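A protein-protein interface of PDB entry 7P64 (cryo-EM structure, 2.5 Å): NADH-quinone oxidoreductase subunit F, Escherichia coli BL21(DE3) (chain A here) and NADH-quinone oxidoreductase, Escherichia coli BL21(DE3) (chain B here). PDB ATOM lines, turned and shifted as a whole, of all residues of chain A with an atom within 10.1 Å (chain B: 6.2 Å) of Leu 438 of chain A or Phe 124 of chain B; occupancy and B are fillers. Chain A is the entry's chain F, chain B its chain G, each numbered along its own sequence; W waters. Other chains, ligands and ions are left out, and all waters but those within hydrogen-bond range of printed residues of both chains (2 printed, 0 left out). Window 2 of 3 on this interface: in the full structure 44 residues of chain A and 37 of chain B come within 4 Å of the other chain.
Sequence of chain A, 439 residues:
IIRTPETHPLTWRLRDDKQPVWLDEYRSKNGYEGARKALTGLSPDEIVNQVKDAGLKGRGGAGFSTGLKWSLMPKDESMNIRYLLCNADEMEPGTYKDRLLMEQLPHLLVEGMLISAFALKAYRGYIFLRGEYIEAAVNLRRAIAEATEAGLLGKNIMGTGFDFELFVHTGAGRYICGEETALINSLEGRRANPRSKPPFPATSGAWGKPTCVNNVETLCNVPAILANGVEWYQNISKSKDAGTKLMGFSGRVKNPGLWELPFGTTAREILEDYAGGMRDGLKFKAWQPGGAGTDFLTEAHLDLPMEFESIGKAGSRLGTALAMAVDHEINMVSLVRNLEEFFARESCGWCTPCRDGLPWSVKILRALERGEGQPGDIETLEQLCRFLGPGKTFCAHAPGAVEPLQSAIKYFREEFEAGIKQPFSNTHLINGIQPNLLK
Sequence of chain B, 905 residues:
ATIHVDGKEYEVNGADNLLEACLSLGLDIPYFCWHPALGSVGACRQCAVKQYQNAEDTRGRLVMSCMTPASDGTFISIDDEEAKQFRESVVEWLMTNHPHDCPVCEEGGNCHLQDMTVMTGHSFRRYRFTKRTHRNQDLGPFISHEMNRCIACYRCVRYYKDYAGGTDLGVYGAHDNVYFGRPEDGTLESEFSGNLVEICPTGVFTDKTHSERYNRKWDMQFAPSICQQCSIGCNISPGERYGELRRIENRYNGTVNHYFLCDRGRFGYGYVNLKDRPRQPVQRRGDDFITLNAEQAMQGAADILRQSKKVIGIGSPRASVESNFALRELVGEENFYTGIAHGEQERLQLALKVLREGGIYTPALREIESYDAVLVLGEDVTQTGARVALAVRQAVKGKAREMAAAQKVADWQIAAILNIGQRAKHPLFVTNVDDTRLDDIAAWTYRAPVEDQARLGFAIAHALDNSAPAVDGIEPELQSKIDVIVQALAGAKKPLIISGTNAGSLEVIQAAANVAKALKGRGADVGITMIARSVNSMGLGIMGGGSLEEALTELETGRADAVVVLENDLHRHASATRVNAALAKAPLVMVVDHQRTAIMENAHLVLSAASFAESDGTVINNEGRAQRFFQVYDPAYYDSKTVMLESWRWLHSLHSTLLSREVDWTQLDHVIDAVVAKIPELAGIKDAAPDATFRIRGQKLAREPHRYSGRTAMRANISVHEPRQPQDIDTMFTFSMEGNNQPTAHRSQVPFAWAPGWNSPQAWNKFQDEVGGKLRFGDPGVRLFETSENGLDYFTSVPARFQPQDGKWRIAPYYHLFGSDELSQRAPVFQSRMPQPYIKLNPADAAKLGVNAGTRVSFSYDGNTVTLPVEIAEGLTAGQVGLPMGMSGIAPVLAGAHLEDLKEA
The side-chain amide oxygen of Gln 383 of chain A sits at hydrogen-bond distance from the guanidinium group of Arg 126 of chain B (3.3 Å). The side-chain amide nitrogen of Asn 426 of chain A is in hydrogen-bond range of the backbone carbonyl oxygen of Arg 125 of chain B (2.6 Å).
NE of Arg 126 of chain B lies within salt-bridge range of OE2 of Glu 92 of chain B, 3.0 Å away.
Among the printed residues, merely in contact across the chains: Trp 360 of chain A with Glu 92 of chain B (3.4 Å), Phe 424 of chain A with Arg 126 of chain B (3.7 Å), Asn 426 of chain A with Arg 126 of chain B (3.5 Å) and Leu 438 of chain A with Phe 124 of chain B (3.97 Å).
Of the printed residues of chain B, Gln 383 of chain A touches Arg 126 (3.3 Å). Printed residues of chain B within 4 Å of Leu 438 of chain A: Phe 124 (3.97 Å). Of the printed residues of chain A, Glu 92 of chain B touches Trp 360 (3.4 Å). No residue of chain A comes within 4 Å of His 122 of chain B. No residue of chain A comes within 4 Å of Ser 123 of chain B. Printed residues of chain A within 4 Å of Phe 124 of chain B: Leu 438. Printed residues of chain A within 4 Å of Arg 125 of chain B: Asn 426. Of the printed residues of chain A, Arg 126 of chain B touches Gln 383, Phe 424 and Asn 426. The nearest printed residue of chain B that does not touch Leu 438 of chain A is Arg 125 of chain B (8.9 Å). The nearest residue of chain A that does not touch Phe 124 of chain B is Phe 424 of chain A (5.1 Å).
Of the 14 printed residues of chain A, 5 touch a printed residue of chain B. Printed residues of chain A that touch a printed residue of chain B: Trp 360, Gln 383, Phe 424, Asn 426 and Leu 438. Hydrophobic or aromatic side chains of chain A within 4 Å of the printed part of chain B: Trp 360, Phe 424 and Leu 438. Of the 7 printed residues of chain B, 4 touch a printed residue of chain A. Hydrophobic or aromatic side chains of chain B that line the printed part of chain A: Phe 124. Among the printed residues, 6 pairs touch across the chains.
Water W1 lies within hydrogen-bond range of the backbone carbonyl oxygen (O) of Arg 126 of chain B and the indole nitrogen (NE1) of Trp 360 of chain A. Water W2 bridges the guanidinium group (NE) of Arg 125 of chain B and the side-chain amide oxygen (OD1) of Asn 426 of chain A.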
ATOM      1  N   TRP A 360     -13.418 -16.031 -21.056  1.00  0.00           N
ATOM      2  CA  TRP A 360     -14.492 -15.096 -20.734  1.00  0.00           C
ATOM      3  C   TRP A 360     -14.425 -14.665 -19.274  1.00  0.00           C
ATOM      4  O   TRP A 360     -14.551 -13.474 -18.965  1.00  0.00           O
ATOM      5  CB  TRP A 360     -15.847 -15.727 -21.054  1.00  0.00           C
ATOM      6  CG  TRP A 360     -16.999 -14.761 -21.128  1.00  0.00           C
ATOM      7  CD1 TRP A 360     -16.975 -13.425 -20.859  1.00  0.00           C
ATOM      8  CD2 TRP A 360     -18.344 -15.065 -21.503  1.00  0.00           C
ATOM      9  NE1 TRP A 360     -18.218 -12.881 -21.034  1.00  0.00           N
ATOM     10  CE2 TRP A 360     -19.079 -13.867 -21.433  1.00  0.00           C
ATOM     11  CE3 TRP A 360     -18.999 -16.235 -21.892  1.00  0.00           C
ATOM     12  CZ2 TRP A 360     -20.433 -13.805 -21.737  1.00  0.00           C
ATOM     13  CZ3 TRP A 360     -20.343 -16.171 -22.191  1.00  0.00           C
ATOM     14  CH2 TRP A 360     -21.045 -14.965 -22.113  1.00  0.00           C
ATOM     15  N   PRO A 375     -23.084  -4.746 -15.165  1.00  0.00           N
ATOM     16  CA  PRO A 375     -24.063  -5.676 -14.585  1.00  0.00           C
ATOM     17  C   PRO A 375     -24.197  -6.954 -15.399  1.00  0.00           C
ATOM     18  O   PRO A 375     -24.168  -6.940 -16.631  1.00  0.00           O
ATOM     19  CB  PRO A 375     -25.363  -4.867 -14.594  1.00  0.00           C
ATOM     20  CG  PRO A 375     -24.920  -3.464 -14.527  1.00  0.00           C
ATOM     21  CD  PRO A 375     -23.648  -3.392 -15.310  1.00  0.00           C
ATOM     22  N   GLY A 376     -24.347  -8.069 -14.688  1.00  0.00           N
ATOM     23  CA  GLY A 376     -24.355  -9.376 -15.297  1.00  0.00           C
ATOM     24  C   GLY A 376     -23.009 -10.064 -15.351  1.00  0.00           C
ATOM     25  O   GLY A 376     -22.945 -11.225 -15.770  1.00  0.00           O
ATOM     26  N   GLN A 383     -22.659 -18.471 -13.534  1.00  0.00           N
ATOM     27  CA  GLN A 383     -23.081 -19.415 -14.565  1.00  0.00           C
ATOM     28  C   GLN A 383     -21.907 -20.248 -15.065  1.00  0.00           C
ATOM     29  O   GLN A 383     -22.054 -21.448 -15.330  1.00  0.00           O
ATOM     30  CB  GLN A 383     -23.739 -18.662 -15.722  1.00  0.00           C
ATOM     31  CG  GLN A 383     -24.283 -19.554 -16.823  1.00  0.00           C
ATOM     32  CD  GLN A 383     -25.440 -18.920 -17.569  1.00  0.00           C
ATOM     33  OE1 GLN A 383     -25.850 -17.801 -17.264  1.00  0.00           O
ATOM     34  NE2 GLN A 383     -25.972 -19.633 -18.554  1.00  0.00           N
ATOM     35  N   PHE A 424     -24.179  -1.656 -18.435  1.00  0.00           N
ATOM     36  CA  PHE A 424     -23.952  -2.692 -19.433  1.00  0.00           C
ATOM     37  C   PHE A 424     -24.220  -2.154 -20.830  1.00  0.00           C
ATOM     38  O   PHE A 424     -25.302  -1.634 -21.113  1.00  0.00           O
ATOM     39  CB  PHE A 424     -24.830  -3.915 -19.175  1.00  0.00           C
ATOM     40  CG  PHE A 424     -24.718  -4.963 -20.248  1.00  0.00           C
ATOM     41  CD1 PHE A 424     -23.561  -5.714 -20.379  1.00  0.00           C
ATOM     42  CD2 PHE A 424     -25.756  -5.181 -21.139  1.00  0.00           C
ATOM     43  CE1 PHE A 424     -23.444  -6.670 -21.370  1.00  0.00           C
ATOM     44  CE2 PHE A 424     -25.645  -6.135 -22.134  1.00  0.00           C
ATOM     45  CZ  PHE A 424     -24.488  -6.880 -22.248  1.00  0.00           C
ATOM     46  N   SER A 425     -23.227  -2.285 -21.704  1.00  0.00           N
ATOM     47  CA  SER A 425     -23.346  -1.852 -23.088  1.00  0.00           C
ATOM     48  C   SER A 425     -22.655  -2.875 -23.970  1.00  0.00           C
ATOM     49  O   SER A 425     -21.463  -3.143 -23.799  1.00  0.00           O
ATOM     50  CB  SER A 425     -22.736  -0.465 -23.296  1.00  0.00           C
ATOM     51  OG  SER A 425     -22.742  -0.111 -24.667  1.00  0.00           O
ATOM     52  N   ASN A 426     -23.408  -3.447 -24.903  1.00  0.00           N
ATOM     53  CA  ASN A 426     -22.878  -4.379 -25.880  1.00  0.00           C
ATOM     54  C   ASN A 426     -22.961  -3.864 -27.305  1.00  0.00           C
ATOM     55  O   ASN A 426     -22.221  -4.350 -28.163  1.00  0.00           O
ATOM     56  CB  ASN A 426     -23.624  -5.719 -25.797  1.00  0.00           C
ATOM     57  CG  ASN A 426     -22.763  -6.882 -26.193  1.00  0.00           C
ATOM     58  OD1 ASN A 426     -21.567  -6.730 -26.410  1.00  0.00           O
ATOM     59  ND2 ASN A 426     -23.365  -8.055 -26.294  1.00  0.00           N
ATOM     60  N   THR A 427     -23.834  -2.901 -27.576  1.00  0.00           N
ATOM     61  CA  THR A 427     -24.063  -2.373 -28.907  1.00  0.00           C
ATOM     62  C   THR A 427     -23.675  -0.906 -28.953  1.00  0.00           C
ATOM     63  O   THR A 427     -23.677  -0.209 -27.935  1.00  0.00           O
ATOM     64  CB  THR A 427     -25.536  -2.510 -29.318  1.00  0.00           C
ATOM     65  OG1 THR A 427     -26.297  -1.475 -28.686  1.00  0.00           O
ATOM     66  CG2 THR A 427     -26.097  -3.848 -28.897  1.00  0.00           C
ATOM     67  N   GLN A 434     -33.662   2.516 -35.136  1.00  0.00           N
ATOM     68  CA  GLN A 434     -34.052   2.689 -33.745  1.00  0.00           C
ATOM     69  C   GLN A 434     -33.868   1.376 -32.993  1.00  0.00           C
ATOM     70  O   GLN A 434     -34.366   0.340 -33.441  1.00  0.00           O
ATOM     71  CB  GLN A 434     -35.496   3.151 -33.646  1.00  0.00           C
ATOM     72  CG  GLN A 434     -35.711   4.583 -34.078  1.00  0.00           C
ATOM     73  CD  GLN A 434     -37.163   4.885 -34.350  1.00  0.00           C
ATOM     74  OE1 GLN A 434     -37.733   4.404 -35.322  1.00  0.00           O
ATOM     75  NE2 GLN A 434     -37.773   5.684 -33.488  1.00  0.00           N
ATOM     76  N   PRO A 435     -33.154   1.376 -31.872  1.00  0.00           N
ATOM     77  CA  PRO A 435     -32.925   0.127 -31.142  1.00  0.00           C
ATOM     78  C   PRO A 435     -34.192  -0.401 -30.489  1.00  0.00           C
ATOM     79  O   PRO A 435     -35.130   0.343 -30.194  1.00  0.00           O
ATOM     80  CB  PRO A 435     -31.886   0.519 -30.089  1.00  0.00           C
ATOM     81  CG  PRO A 435     -32.104   1.970 -29.884  1.00  0.00           C
ATOM     82  CD  PRO A 435     -32.512   2.526 -31.214  1.00  0.00           C
ATOM     83  N   ASN A 436     -34.210  -1.713 -30.274  1.00  0.00           N
ATOM     84  CA  ASN A 436     -35.270  -2.362 -29.512  1.00  0.00           C
ATOM     85  C   ASN A 436     -34.985  -2.133 -28.035  1.00  0.00           C
ATOM     86  O   ASN A 436     -34.178  -2.837 -27.428  1.00  0.00           O
ATOM     87  CB  ASN A 436     -35.340  -3.846 -29.843  1.00  0.00           C
ATOM     88  CG  ASN A 436     -36.700  -4.437 -29.575  1.00  0.00           C
ATOM     89  OD1 ASN A 436     -37.712  -3.755 -29.689  1.00  0.00           O
ATOM     90  ND2 ASN A 436     -36.733  -5.711 -29.210  1.00  0.00           N
ATOM     91  N   LEU A 437     -35.653  -1.142 -27.452  1.00  0.00           N
ATOM     92  CA  LEU A 437     -35.391  -0.718 -26.078  1.00  0.00           C
ATOM     93  C   LEU A 437     -36.001  -1.733 -25.123  1.00  0.00           C
ATOM     94  O   LEU A 437     -37.143  -1.599 -24.684  1.00  0.00           O
ATOM     95  CB  LEU A 437     -35.952   0.676 -25.832  1.00  0.00           C
ATOM     96  CG  LEU A 437     -35.394   1.794 -26.712  1.00  0.00           C
ATOM     97  CD1 LEU A 437     -36.219   3.061 -26.553  1.00  0.00           C
ATOM     98  CD2 LEU A 437     -33.934   2.052 -26.384  1.00  0.00           C
ATOM     99  N   LEU A 438     -35.227  -2.762 -24.793  1.00  0.00           N
ATOM    100  CA  LEU A 438     -35.690  -3.776 -23.854  1.00  0.00           C
ATOM    101  C   LEU A 438     -35.710  -3.214 -22.438  1.00  0.00           C
ATOM    102  O   LEU A 438     -34.730  -2.619 -21.980  1.00  0.00           O
ATOM    103  CB  LEU A 438     -34.796  -5.011 -23.920  1.00  0.00           C
ATOM    104  CG  LEU A 438     -35.113  -6.031 -25.015  1.00  0.00           C
ATOM    105  CD1 LEU A 438     -33.933  -6.964 -25.232  1.00  0.00           C
ATOM    106  CD2 LEU A 438     -36.366  -6.818 -24.671  1.00  0.00           C
ATOM    107  N   LYS A 439     -36.827  -3.407 -21.746  1.00  0.00           N
ATOM    108  CA  LYS A 439     -36.968  -2.942 -20.373  1.00  0.00           C
ATOM    109  C   LYS A 439     -36.765  -4.090 -19.388  1.00  0.00           C
ATOM    110  O   LYS A 439     -36.371  -3.880 -18.241  1.00  0.00           O
ATOM    111  CB  LYS A 439     -38.341  -2.298 -20.161  1.00  0.00           C
ATOM    112  CG  LYS A 439     -38.584  -1.054 -21.007  1.00  0.00           C
ATOM    113  CD  LYS A 439     -37.712   0.105 -20.551  1.00  0.00           C
ATOM    114  CE  LYS A 439     -38.082   1.398 -21.263  1.00  0.00           C
ATOM    115  NZ  LYS A 439     -37.619   1.424 -22.678  1.00  0.00           N
ATOM    116  N   GLU B  92     -23.288 -20.455 -26.923  1.00  0.00           N
ATOM    117  CA  GLU B  92     -22.872 -19.095 -26.590  1.00  0.00           C
ATOM    118  C   GLU B  92     -21.358 -18.979 -26.471  1.00  0.00           C
ATOM    119  O   GLU B  92     -20.769 -17.993 -26.929  1.00  0.00           O
ATOM    120  CB  GLU B  92     -23.544 -18.658 -25.290  1.00  0.00           C
ATOM    121  CG  GLU B  92     -23.141 -17.282 -24.823  1.00  0.00           C
ATOM    122  CD  GLU B  92     -23.973 -16.794 -23.665  1.00  0.00           C
ATOM    123  OE1 GLU B  92     -24.550 -17.634 -22.946  1.00  0.00           O
ATOM    124  OE2 GLU B  92     -24.062 -15.566 -23.481  1.00  0.00           O
ATOM    125  N   GLY B 121     -31.733 -21.995 -29.524  1.00  0.00           N
ATOM    126  CA  GLY B 121     -32.461 -20.798 -29.162  1.00  0.00           C
ATOM    127  C   GLY B 121     -31.604 -19.647 -28.697  1.00  0.00           C
ATOM    128  O   GLY B 121     -32.094 -18.787 -27.962  1.00  0.00           O
ATOM    129  N   HIS B 122     -30.340 -19.601 -29.100  1.00  0.00           N
ATOM    130  CA  HIS B 122     -29.415 -18.561 -28.667  1.00  0.00           C
ATOM    131  C   HIS B 122     -29.348 -17.479 -29.738  1.00  0.00           C
ATOM    132  O   HIS B 122     -28.791 -17.696 -30.817  1.00  0.00           O
ATOM    133  CB  HIS B 122     -28.034 -19.150 -28.398  1.00  0.00           C
ATOM    134  CG  HIS B 122     -27.000 -18.124 -28.061  1.00  0.00           C
ATOM    135  ND1 HIS B 122     -26.989 -17.449 -26.862  1.00  0.00           N
ATOM    136  CD2 HIS B 122     -25.951 -17.649 -28.771  1.00  0.00           C
ATOM    137  CE1 HIS B 122     -25.974 -16.606 -26.844  1.00  0.00           C
ATOM    138  NE2 HIS B 122     -25.330 -16.706 -27.992  1.00  0.00           N
ATOM    139  N   SER B 123     -29.910 -16.311 -29.435  1.00  0.00           N
ATOM    140  CA  SER B 123     -29.886 -15.187 -30.356  1.00  0.00           C
ATOM    141  C   SER B 123     -29.479 -13.880 -29.697  1.00  0.00           C
ATOM    142  O   SER B 123     -29.428 -12.854 -30.380  1.00  0.00           O
ATOM    143  CB  SER B 123     -31.258 -15.009 -31.020  1.00  0.00           C
ATOM    144  OG  SER B 123     -32.286 -14.936 -30.051  1.00  0.00           O
ATOM    145  N   PHE B 124     -29.185 -13.883 -28.402  1.00  0.00           N
ATOM    146  CA  PHE B 124     -28.840 -12.678 -27.666  1.00  0.00           C
ATOM    147  C   PHE B 124     -27.385 -12.750 -27.229  1.00  0.00           C
ATOM    148  O   PHE B 124     -26.977 -13.715 -26.577  1.00  0.00           O
ATOM    149  CB  PHE B 124     -29.753 -12.506 -26.452  1.00  0.00           C
ATOM    150  CG  PHE B 124     -29.703 -11.138 -25.845  1.00  0.00           C
ATOM    151  CD1 PHE B 124     -30.527 -10.132 -26.314  1.00  0.00           C
ATOM    152  CD2 PHE B 124     -28.835 -10.857 -24.803  1.00  0.00           C
ATOM    153  CE1 PHE B 124     -30.489  -8.874 -25.756  1.00  0.00           C
ATOM    154  CE2 PHE B 124     -28.788  -9.600 -24.246  1.00  0.00           C
ATOM    155  CZ  PHE B 124     -29.615  -8.607 -24.724  1.00  0.00           C
ATOM    156  N   ARG B 125     -26.616 -11.725 -27.569  1.00  0.00           N
ATOM    157  CA  ARG B 125     -25.199 -11.662 -27.245  1.00  0.00           C
ATOM    158  C   ARG B 125     -25.002 -10.772 -26.027  1.00  0.00           C
ATOM    159  O   ARG B 125     -25.424  -9.612 -26.030  1.00  0.00           O
ATOM    160  CB  ARG B 125     -24.402 -11.126 -28.431  1.00  0.00           C
ATOM    161  CG  ARG B 125     -22.899 -11.116 -28.241  1.00  0.00           C
ATOM    162  CD  ARG B 125     -22.213 -10.691 -29.522  1.00  0.00           C
ATOM    163  NE  ARG B 125     -20.760 -10.744 -29.437  1.00  0.00           N
ATOM    164  CZ  ARG B 125     -20.032 -11.820 -29.696  1.00  0.00           C
ATOM    165  NH1 ARG B 125     -20.592 -12.973 -30.012  1.00  0.00           N
ATOM    166  NH2 ARG B 125     -18.708 -11.737 -29.637  1.00  0.00           N
ATOM    167  N   ARG B 126     -24.360 -11.308 -24.991  1.00  0.00           N
ATOM    168  CA  ARG B 126     -23.927 -10.497 -23.866  1.00  0.00           C
ATOM    169  C   ARG B 126     -22.415 -10.398 -23.749  1.00  0.00           C
ATOM    170  O   ARG B 126     -21.926  -9.606 -22.937  1.00  0.00           O
ATOM    171  CB  ARG B 126     -24.505 -11.032 -22.549  1.00  0.00           C
ATOM    172  CG  ARG B 126     -24.508 -12.531 -22.420  1.00  0.00           C
ATOM    173  CD  ARG B 126     -25.494 -12.973 -21.355  1.00  0.00           C
ATOM    174  NE  ARG B 126     -25.400 -14.401 -21.083  1.00  0.00           N
ATOM    175  CZ  ARG B 126     -24.696 -14.926 -20.091  1.00  0.00           C
ATOM    176  NH1 ARG B 126     -24.003 -14.168 -19.259  1.00  0.00           N
ATOM    177  NH2 ARG B 126     -24.686 -16.245 -19.932  1.00  0.00           N
HETATM  178  O   HOH W   1     -19.804  -9.818 -21.300  1.00  0.00           O
HETATM  179  O   HOH W   2     -19.883  -7.908 -28.882  1.00  0.00           O
